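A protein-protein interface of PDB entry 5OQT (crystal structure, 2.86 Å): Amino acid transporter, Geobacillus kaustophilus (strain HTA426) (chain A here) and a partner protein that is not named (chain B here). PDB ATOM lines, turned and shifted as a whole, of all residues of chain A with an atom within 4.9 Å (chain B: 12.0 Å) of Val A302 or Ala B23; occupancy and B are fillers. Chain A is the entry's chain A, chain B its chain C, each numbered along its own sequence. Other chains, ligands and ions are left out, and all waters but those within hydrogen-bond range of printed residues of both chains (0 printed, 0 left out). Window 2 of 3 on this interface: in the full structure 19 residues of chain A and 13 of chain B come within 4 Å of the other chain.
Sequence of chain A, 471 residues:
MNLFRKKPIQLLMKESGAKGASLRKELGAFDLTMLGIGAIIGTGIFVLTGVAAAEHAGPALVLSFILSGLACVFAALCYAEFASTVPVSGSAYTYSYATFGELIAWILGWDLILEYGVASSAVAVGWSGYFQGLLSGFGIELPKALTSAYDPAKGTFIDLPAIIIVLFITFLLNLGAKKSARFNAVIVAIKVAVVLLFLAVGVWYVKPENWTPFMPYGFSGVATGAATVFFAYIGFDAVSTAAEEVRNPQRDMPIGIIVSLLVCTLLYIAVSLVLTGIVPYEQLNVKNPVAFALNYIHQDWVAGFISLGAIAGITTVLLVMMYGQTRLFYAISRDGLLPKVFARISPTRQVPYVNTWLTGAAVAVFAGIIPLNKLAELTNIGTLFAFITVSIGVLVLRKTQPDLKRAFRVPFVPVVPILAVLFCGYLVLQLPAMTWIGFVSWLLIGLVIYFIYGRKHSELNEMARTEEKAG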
ATOM      1  N   LEU A 197      16.633 -18.765 -17.675  1.00  0.00           N
ATOM      2  CA  LEU A 197      16.251 -19.079 -19.042  1.00  0.00           C
ATOM      3  C   LEU A 197      17.466 -19.019 -19.968  1.00  0.00           C
ATOM      4  O   LEU A 197      17.670 -19.961 -20.735  1.00  0.00           O
ATOM      5  CB  LEU A 197      15.125 -18.159 -19.524  1.00  0.00           C
ATOM      6  CG  LEU A 197      14.486 -18.511 -20.872  1.00  0.00           C
ATOM      7  CD1 LEU A 197      13.883 -19.912 -20.861  1.00  0.00           C
ATOM      8  CD2 LEU A 197      13.419 -17.523 -21.228  1.00  0.00           C
ATOM      9  N   VAL A 201      18.772 -22.479 -21.728  1.00  0.00           N
ATOM     10  CA  VAL A 201      18.714 -22.535 -23.194  1.00  0.00           C
ATOM     11  C   VAL A 201      20.126 -22.462 -23.777  1.00  0.00           C
ATOM     12  O   VAL A 201      20.448 -23.186 -24.720  1.00  0.00           O
ATOM     13  CB  VAL A 201      17.759 -21.447 -23.784  1.00  0.00           C
ATOM     14  CG1 VAL A 201      17.785 -21.433 -25.309  1.00  0.00           C
ATOM     15  CG2 VAL A 201      16.324 -21.636 -23.287  1.00  0.00           C
ATOM     16  N   LEU A 294      22.240 -14.939 -27.362  1.00  0.00           N
ATOM     17  CA  LEU A 294      21.067 -15.688 -27.801  1.00  0.00           C
ATOM     18  C   LEU A 294      20.801 -15.495 -29.292  1.00  0.00           C
ATOM     19  O   LEU A 294      20.458 -16.468 -29.965  1.00  0.00           O
ATOM     20  CB  LEU A 294      19.835 -15.345 -26.965  1.00  0.00           C
ATOM     21  CG  LEU A 294      19.749 -16.007 -25.600  1.00  0.00           C
ATOM     22  CD1 LEU A 294      18.976 -15.151 -24.650  1.00  0.00           C
ATOM     23  CD2 LEU A 294      19.151 -17.403 -25.691  1.00  0.00           C
ATOM     24  N   GLN A 299      18.531 -17.889 -31.375  1.00  0.00           N
ATOM     25  CA  GLN A 299      17.417 -18.017 -30.437  1.00  0.00           C
ATOM     26  C   GLN A 299      16.793 -16.627 -30.260  1.00  0.00           C
ATOM     27  O   GLN A 299      16.729 -16.098 -29.154  1.00  0.00           O
ATOM     28  CB  GLN A 299      17.909 -18.604 -29.102  1.00  0.00           C
ATOM     29  CG  GLN A 299      17.964 -20.132 -29.058  1.00  0.00           C
ATOM     30  CD  GLN A 299      16.611 -20.824 -29.064  1.00  0.00           C
ATOM     31  OE1 GLN A 299      15.537 -20.203 -28.954  1.00  0.00           O
ATOM     32  NE2 GLN A 299      16.641 -22.143 -29.189  1.00  0.00           N
ATOM     33  N   ASP A 300      16.360 -16.029 -31.379  1.00  0.00           N
ATOM     34  CA  ASP A 300      15.825 -14.667 -31.486  1.00  0.00           C
ATOM     35  C   ASP A 300      14.648 -14.345 -30.562  1.00  0.00           C
ATOM     36  O   ASP A 300      14.604 -13.249 -30.000  1.00  0.00           O
ATOM     37  CB  ASP A 300      15.456 -14.361 -32.947  1.00  0.00           C
ATOM     38  CG  ASP A 300      16.653 -14.278 -33.880  1.00  0.00           C
ATOM     39  OD1 ASP A 300      17.565 -15.130 -33.759  1.00  0.00           O
ATOM     40  OD2 ASP A 300      16.660 -13.384 -34.760  1.00  0.00           O
ATOM     41  N   TRP A 301      13.705 -15.291 -30.423  1.00  0.00           N
ATOM     42  CA  TRP A 301      12.490 -15.185 -29.608  1.00  0.00           C
ATOM     43  C   TRP A 301      12.817 -15.129 -28.095  1.00  0.00           C
ATOM     44  O   TRP A 301      12.303 -14.255 -27.391  1.00  0.00           O
ATOM     45  CB  TRP A 301      11.585 -16.380 -29.933  1.00  0.00           C
ATOM     46  CG  TRP A 301      10.107 -16.132 -29.892  1.00  0.00           C
ATOM     47  CD1 TRP A 301       9.427 -15.316 -29.029  1.00  0.00           C
ATOM     48  CD2 TRP A 301       9.109 -16.839 -30.648  1.00  0.00           C
ATOM     49  NE1 TRP A 301       8.070 -15.428 -29.242  1.00  0.00           N
ATOM     50  CE2 TRP A 301       7.845 -16.370 -30.219  1.00  0.00           C
ATOM     51  CE3 TRP A 301       9.161 -17.831 -31.653  1.00  0.00           C
ATOM     52  CZ2 TRP A 301       6.642 -16.850 -30.766  1.00  0.00           C
ATOM     53  CZ3 TRP A 301       7.970 -18.300 -32.196  1.00  0.00           C
ATOM     54  CH2 TRP A 301       6.731 -17.810 -31.757  1.00  0.00           C
ATOM     55  N   VAL A 302      13.698 -16.043 -27.623  1.00  0.00           N
ATOM     56  CA  VAL A 302      14.189 -16.145 -26.246  1.00  0.00           C
ATOM     57  C   VAL A 302      15.009 -14.890 -25.886  1.00  0.00           C
ATOM     58  O   VAL A 302      14.930 -14.421 -24.740  1.00  0.00           O
ATOM     59  CB  VAL A 302      14.984 -17.462 -26.025  1.00  0.00           C
ATOM     60  CG1 VAL A 302      15.565 -17.542 -24.616  1.00  0.00           C
ATOM     61  CG2 VAL A 302      14.107 -18.678 -26.293  1.00  0.00           C
ATOM     62  N   ALA A 303      15.769 -14.347 -26.869  1.00  0.00           N
ATOM     63  CA  ALA A 303      16.589 -13.138 -26.752  1.00  0.00           C
ATOM     64  C   ALA A 303      15.745 -11.886 -26.483  1.00  0.00           C
ATOM     65  O   ALA A 303      16.149 -11.050 -25.675  1.00  0.00           O
ATOM     66  CB  ALA A 303      17.426 -12.943 -28.007  1.00  0.00           C
ATOM     67  N   GLY A 304      14.602 -11.765 -27.163  1.00  0.00           N
ATOM     68  CA  GLY A 304      13.679 -10.649 -26.981  1.00  0.00           C
ATOM     69  C   GLY A 304      12.982 -10.745 -25.636  1.00  0.00           C
ATOM     70  O   GLY A 304      12.806  -9.744 -24.933  1.00  0.00           O
ATOM     71  N   PHE A 305      12.620 -11.981 -25.263  1.00  0.00           N
ATOM     72  CA  PHE A 305      11.998 -12.348 -24.000  1.00  0.00           C
ATOM     73  C   PHE A 305      12.949 -12.026 -22.810  1.00  0.00           C
ATOM     74  O   PHE A 305      12.496 -11.528 -21.776  1.00  0.00           O
ATOM     75  CB  PHE A 305      11.602 -13.832 -24.058  1.00  0.00           C
ATOM     76  CG  PHE A 305      10.527 -14.257 -23.094  1.00  0.00           C
ATOM     77  CD1 PHE A 305      10.739 -15.310 -22.215  1.00  0.00           C
ATOM     78  CD2 PHE A 305       9.298 -13.604 -23.063  1.00  0.00           C
ATOM     79  CE1 PHE A 305       9.742 -15.702 -21.315  1.00  0.00           C
ATOM     80  CE2 PHE A 305       8.306 -13.983 -22.148  1.00  0.00           C
ATOM     81  CZ  PHE A 305       8.538 -15.025 -21.272  1.00  0.00           C
ATOM     82  N   ILE A 306      14.267 -12.249 -22.991  1.00  0.00           N
ATOM     83  CA  ILE A 306      15.291 -11.902 -21.997  1.00  0.00           C
ATOM     84  C   ILE A 306      15.513 -10.375 -21.989  1.00  0.00           C
ATOM     85  O   ILE A 306      15.757  -9.810 -20.925  1.00  0.00           O
ATOM     86  CB  ILE A 306      16.593 -12.751 -22.160  1.00  0.00           C
ATOM     87  CG1 ILE A 306      16.530 -13.973 -21.225  1.00  0.00           C
ATOM     88  CG2 ILE A 306      17.884 -11.942 -21.906  1.00  0.00           C
ATOM     89  CD1 ILE A 306      16.832 -15.262 -21.807  1.00  0.00           C
ATOM     90  N   LEU B  12       8.156 -17.660 -12.005  1.00  0.00           N
ATOM     91  CA  LEU B  12       9.355 -18.321 -12.530  1.00  0.00           C
ATOM     92  C   LEU B  12       8.875 -19.410 -13.493  1.00  0.00           C
ATOM     93  O   LEU B  12       9.290 -19.405 -14.648  1.00  0.00           O
ATOM     94  CB  LEU B  12      10.232 -18.991 -11.450  1.00  0.00           C
ATOM     95  CG  LEU B  12      10.818 -18.187 -10.300  1.00  0.00           C
ATOM     96  CD1 LEU B  12      11.576 -19.107  -9.395  1.00  0.00           C
ATOM     97  CD2 LEU B  12      11.757 -17.084 -10.781  1.00  0.00           C
ATOM     98  N   ILE B  14       5.936 -19.818 -15.013  1.00  0.00           N
ATOM     99  CA  ILE B  14       5.203 -19.289 -16.173  1.00  0.00           C
ATOM    100  C   ILE B  14       6.197 -18.882 -17.271  1.00  0.00           C
ATOM    101  O   ILE B  14       6.029 -19.296 -18.419  1.00  0.00           O
ATOM    102  CB  ILE B  14       4.216 -18.159 -15.759  1.00  0.00           C
ATOM    103  CG1 ILE B  14       2.949 -18.762 -15.105  1.00  0.00           C
ATOM    104  CG2 ILE B  14       3.842 -17.270 -16.942  1.00  0.00           C
ATOM    105  CD1 ILE B  14       2.256 -17.881 -14.007  1.00  0.00           C
ATOM    106  N   ILE B  15       7.247 -18.123 -16.896  1.00  0.00           N
ATOM    107  CA  ILE B  15       8.326 -17.672 -17.780  1.00  0.00           C
ATOM    108  C   ILE B  15       9.181 -18.884 -18.250  1.00  0.00           C
ATOM    109  O   ILE B  15       9.529 -18.960 -19.427  1.00  0.00           O
ATOM    110  CB  ILE B  15       9.165 -16.558 -17.092  1.00  0.00           C
ATOM    111  CG1 ILE B  15       8.321 -15.304 -16.842  1.00  0.00           C
ATOM    112  CG2 ILE B  15      10.415 -16.210 -17.895  1.00  0.00           C
ATOM    113  CD1 ILE B  15       8.766 -14.485 -15.657  1.00  0.00           C
ATOM    114  N   LEU B  16       9.494 -19.829 -17.348  1.00  0.00           N
ATOM    115  CA  LEU B  16      10.253 -21.023 -17.717  1.00  0.00           C
ATOM    116  C   LEU B  16       9.426 -21.957 -18.601  1.00  0.00           C
ATOM    117  O   LEU B  16      10.000 -22.718 -19.373  1.00  0.00           O
ATOM    118  CB  LEU B  16      10.831 -21.772 -16.508  1.00  0.00           C
ATOM    119  CG  LEU B  16      11.960 -21.083 -15.755  1.00  0.00           C
ATOM    120  CD1 LEU B  16      12.108 -21.669 -14.363  1.00  0.00           C
ATOM    121  CD2 LEU B  16      13.273 -21.152 -16.511  1.00  0.00           C
ATOM    122  N   PHE B  17       8.086 -21.889 -18.518  1.00  0.00           N
ATOM    123  CA  PHE B  17       7.235 -22.689 -19.391  1.00  0.00           C
ATOM    124  C   PHE B  17       7.264 -22.045 -20.791  1.00  0.00           C
ATOM    125  O   PHE B  17       7.595 -22.722 -21.763  1.00  0.00           O
ATOM    126  CB  PHE B  17       5.801 -22.768 -18.837  1.00  0.00           C
ATOM    127  CG  PHE B  17       4.805 -23.480 -19.718  1.00  0.00           C
ATOM    128  CD1 PHE B  17       4.680 -24.863 -19.677  1.00  0.00           C
ATOM    129  CD2 PHE B  17       3.968 -22.765 -20.566  1.00  0.00           C
ATOM    130  CE1 PHE B  17       3.752 -25.521 -20.489  1.00  0.00           C
ATOM    131  CE2 PHE B  17       3.043 -23.423 -21.382  1.00  0.00           C
ATOM    132  CZ  PHE B  17       2.942 -24.797 -21.339  1.00  0.00           C
ATOM    133  N   SER B  18       6.966 -20.728 -20.867  1.00  0.00           N
ATOM    134  CA  SER B  18       6.919 -19.923 -22.093  1.00  0.00           C
ATOM    135  C   SER B  18       8.271 -19.855 -22.805  1.00  0.00           C
ATOM    136  O   SER B  18       8.325 -19.883 -24.038  1.00  0.00           O
ATOM    137  CB  SER B  18       6.414 -18.517 -21.782  1.00  0.00           C
ATOM    138  OG  SER B  18       5.198 -18.547 -21.052  1.00  0.00           O
ATOM    139  N   GLY B  19       9.338 -19.792 -22.016  1.00  0.00           N
ATOM    140  CA  GLY B  19      10.708 -19.743 -22.500  1.00  0.00           C
ATOM    141  C   GLY B  19      11.126 -21.040 -23.148  1.00  0.00           C
ATOM    142  O   GLY B  19      11.528 -21.036 -24.310  1.00  0.00           O
ATOM    143  N   PHE B  20      10.979 -22.170 -22.422  1.00  0.00           N
ATOM    144  CA  PHE B  20      11.321 -23.511 -22.918  1.00  0.00           C
ATOM    145  C   PHE B  20      10.487 -23.849 -24.170  1.00  0.00           C
ATOM    146  O   PHE B  20      10.967 -24.544 -25.071  1.00  0.00           O
ATOM    147  CB  PHE B  20      11.094 -24.581 -21.827  1.00  0.00           C
ATOM    148  CG  PHE B  20      11.989 -24.619 -20.603  1.00  0.00           C
ATOM    149  CD1 PHE B  20      12.862 -23.570 -20.316  1.00  0.00           C
ATOM    150  CD2 PHE B  20      11.905 -25.670 -19.695  1.00  0.00           C
ATOM    151  CE1 PHE B  20      13.686 -23.614 -19.190  1.00  0.00           C
ATOM    152  CE2 PHE B  20      12.706 -25.695 -18.552  1.00  0.00           C
ATOM    153  CZ  PHE B  20      13.597 -24.674 -18.312  1.00  0.00           C
ATOM    154  N   LEU B  21       9.246 -23.339 -24.223  1.00  0.00           N
ATOM    155  CA  LEU B  21       8.330 -23.521 -25.340  1.00  0.00           C
ATOM    156  C   LEU B  21       8.871 -22.808 -26.597  1.00  0.00           C
ATOM    157  O   LEU B  21       9.080 -23.460 -27.622  1.00  0.00           O
ATOM    158  CB  LEU B  21       6.953 -22.970 -24.955  1.00  0.00           C
ATOM    159  CG  LEU B  21       5.746 -23.629 -25.590  1.00  0.00           C
ATOM    160  CD1 LEU B  21       5.500 -25.006 -24.997  1.00  0.00           C
ATOM    161  CD2 LEU B  21       4.505 -22.771 -25.385  1.00  0.00           C
ATOM    162  N   ALA B  22       9.152 -21.487 -26.497  1.00  0.00           N
ATOM    163  CA  ALA B  22       9.678 -20.670 -27.594  1.00  0.00           C
ATOM    164  C   ALA B  22      11.059 -21.141 -28.079  1.00  0.00           C
ATOM    165  O   ALA B  22      11.362 -21.012 -29.269  1.00  0.00           O
ATOM    166  CB  ALA B  22       9.735 -19.212 -27.176  1.00  0.00           C
ATOM    167  N   ALA B  23      11.884 -21.693 -27.157  1.00  0.00           N
ATOM    168  CA  ALA B  23      13.231 -22.201 -27.432  1.00  0.00           C
ATOM    169  C   ALA B  23      13.190 -23.427 -28.320  1.00  0.00           C
ATOM    170  O   ALA B  23      14.079 -23.621 -29.149  1.00  0.00           O
ATOM    171  CB  ALA B  23      13.942 -22.534 -26.129  1.00  0.00           C
ATOM    172  N   TYR B  24      12.162 -24.258 -28.132  1.00  0.00           N
ATOM    173  CA  TYR B  24      11.936 -25.490 -28.873  1.00  0.00           C
ATOM    174  C   TYR B  24      11.642 -25.184 -30.331  1.00  0.00           C
ATOM    175  O   TYR B  24      12.094 -25.918 -31.203  1.00  0.00           O
ATOM    176  CB  TYR B  24      10.785 -26.276 -28.229  1.00  0.00           C
ATOM    177  CG  TYR B  24      10.562 -27.636 -28.840  1.00  0.00           C
ATOM    178  CD1 TYR B  24      11.362 -28.719 -28.489  1.00  0.00           C
ATOM    179  CD2 TYR B  24       9.537 -27.848 -29.758  1.00  0.00           C
ATOM    180  CE1 TYR B  24      11.161 -29.975 -29.051  1.00  0.00           C
ATOM    181  CE2 TYR B  24       9.333 -29.098 -30.333  1.00  0.00           C
ATOM    182  CZ  TYR B  24      10.142 -30.160 -29.969  1.00  0.00           C
ATOM    183  OH  TYR B  24       9.943 -31.394 -30.528  1.00  0.00           O
ATOM    184  N   PHE B  25      10.915 -24.089 -30.593  1.00  0.00           N
ATOM    185  CA  PHE B  25      10.552 -23.648 -31.936  1.00  0.00           C
ATOM    186  C   PHE B  25      11.530 -22.596 -32.485  1.00  0.00           C
ATOM    187  O   PHE B  25      11.185 -21.417 -32.630  1.00  0.00           O
ATOM    188  CB  PHE B  25       9.092 -23.177 -31.960  1.00  0.00           C
ATOM    189  CG  PHE B  25       8.133 -24.252 -31.506  1.00  0.00           C
ATOM    190  CD1 PHE B  25       7.882 -25.366 -32.301  1.00  0.00           C
ATOM    191  CD2 PHE B  25       7.491 -24.158 -30.280  1.00  0.00           C
ATOM    192  CE1 PHE B  25       7.003 -26.362 -31.879  1.00  0.00           C
ATOM    193  CE2 PHE B  25       6.613 -25.159 -29.857  1.00  0.00           C
ATOM    194  CZ  PHE B  25       6.368 -26.249 -30.665  1.00  0.00           C
ATOM    195  N   SER B  26      12.772 -23.044 -32.763  1.00  0.00           N
ATOM    196  CA  SER B  26      13.880 -22.237 -33.282  1.00  0.00           C
ATOM    197  C   SER B  26      14.874 -23.150 -34.002  1.00  0.00           C
ATOM    198  O   SER B  26      15.020 -24.312 -33.607  1.00  0.00           O
ATOM    199  CB  SER B  26      14.578 -21.496 -32.142  1.00  0.00           C
ATOM    200  OG  SER B  26      15.822 -20.943 -32.544  1.00  0.00           O
ATOM    201  N   HIS B  27      15.566 -22.609 -35.038  1.00  0.00           N
ATOM    202  CA  HIS B  27      16.564 -23.295 -35.874  1.00  0.00           C
ATOM    203  C   HIS B  27      17.798 -23.725 -35.074  1.00  0.00           C
ATOM    204  O   HIS B  27      18.431 -24.726 -35.411  1.00  0.00           O
ATOM    205  CB  HIS B  27      16.953 -22.407 -37.079  1.00  0.00           C
ATOM    206  CG  HIS B  27      18.244 -22.777 -37.759  1.00  0.00           C
ATOM    207  ND1 HIS B  27      19.393 -22.017 -37.594  1.00  0.00           N
ATOM    208  CD2 HIS B  27      18.529 -23.825 -38.570  1.00  0.00           C
ATOM    209  CE1 HIS B  27      20.328 -22.617 -38.312  1.00  0.00           C
ATOM    210  NE2 HIS B  27      19.858 -23.709 -38.916  1.00  0.00           N
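Of chain B, only Gly B19 (3.6 Å) and Phe B20 (3.8 Å) come within 4 Å of Leu A197. Val A201 touches one residue of chain B. Gln A299 touches just these residues of chain B: Ala B23 and Ser B26. Printed residues of chain B within 4 Å of Val A302: Ala B23 (3.8 Å). No residue of chain B comes within 4 Å of Ala A303. Printed residues of chain A within 4 Å of Gly B19: Leu A197 (3.6 Å). Of the printed residues of chain A, Phe B20 touches Leu A197. Ala B23 touches just these residues of chain A: Val A201, Gln A299 and Val A302. The nearest printed residue of chain B that does not touch Val A302 is Gly B19 (4.02 Å). The nearest printed residue of chain A that does not touch Ala B23 is Leu A197 (5.9 Å). The nearest printed residue of chain A that does not touch Ser B26 is Asp A300 (5.1 Å).
The side-chain amide nitrogen of Gln A299 is in hydrogen-bond range of the backbone carbonyl oxygen of Ala B23 (3.0 Å).
The backbone NH of Gln A299 lies within hydrogen-bond range of the backbone carbonyl oxygen of Leu A294, 2.8 Å away.
Gly B19 touches Leu A197 (CA to CD1, 3.6 Å). Phe B20 touches Leu A197 (CD1 to CD1, 3.8 Å). Ala B23 touches Val A201. Gln A299 touches Ser B26. CA of Ala B23 touches CG2 of Val A302, at 3.8 Å. Ile B15 touches Phe A305.
Of the 15 printed residues of chain B, 5 touch a printed residue of chain A. Printed residues of chain B that touch a printed residue of chain A: Ile B15, Gly B19, Phe B20, Ala B23 and Ser B26. Hydrophobic or aromatic side chains of chain B that line the printed part of chain A: Ile B15, Phe B20 and Ala B23. Among the printed residues, no Asp or Glu carboxylate lies within 4 Å of a Lys or Arg side-chain nitrogen of the other chain.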
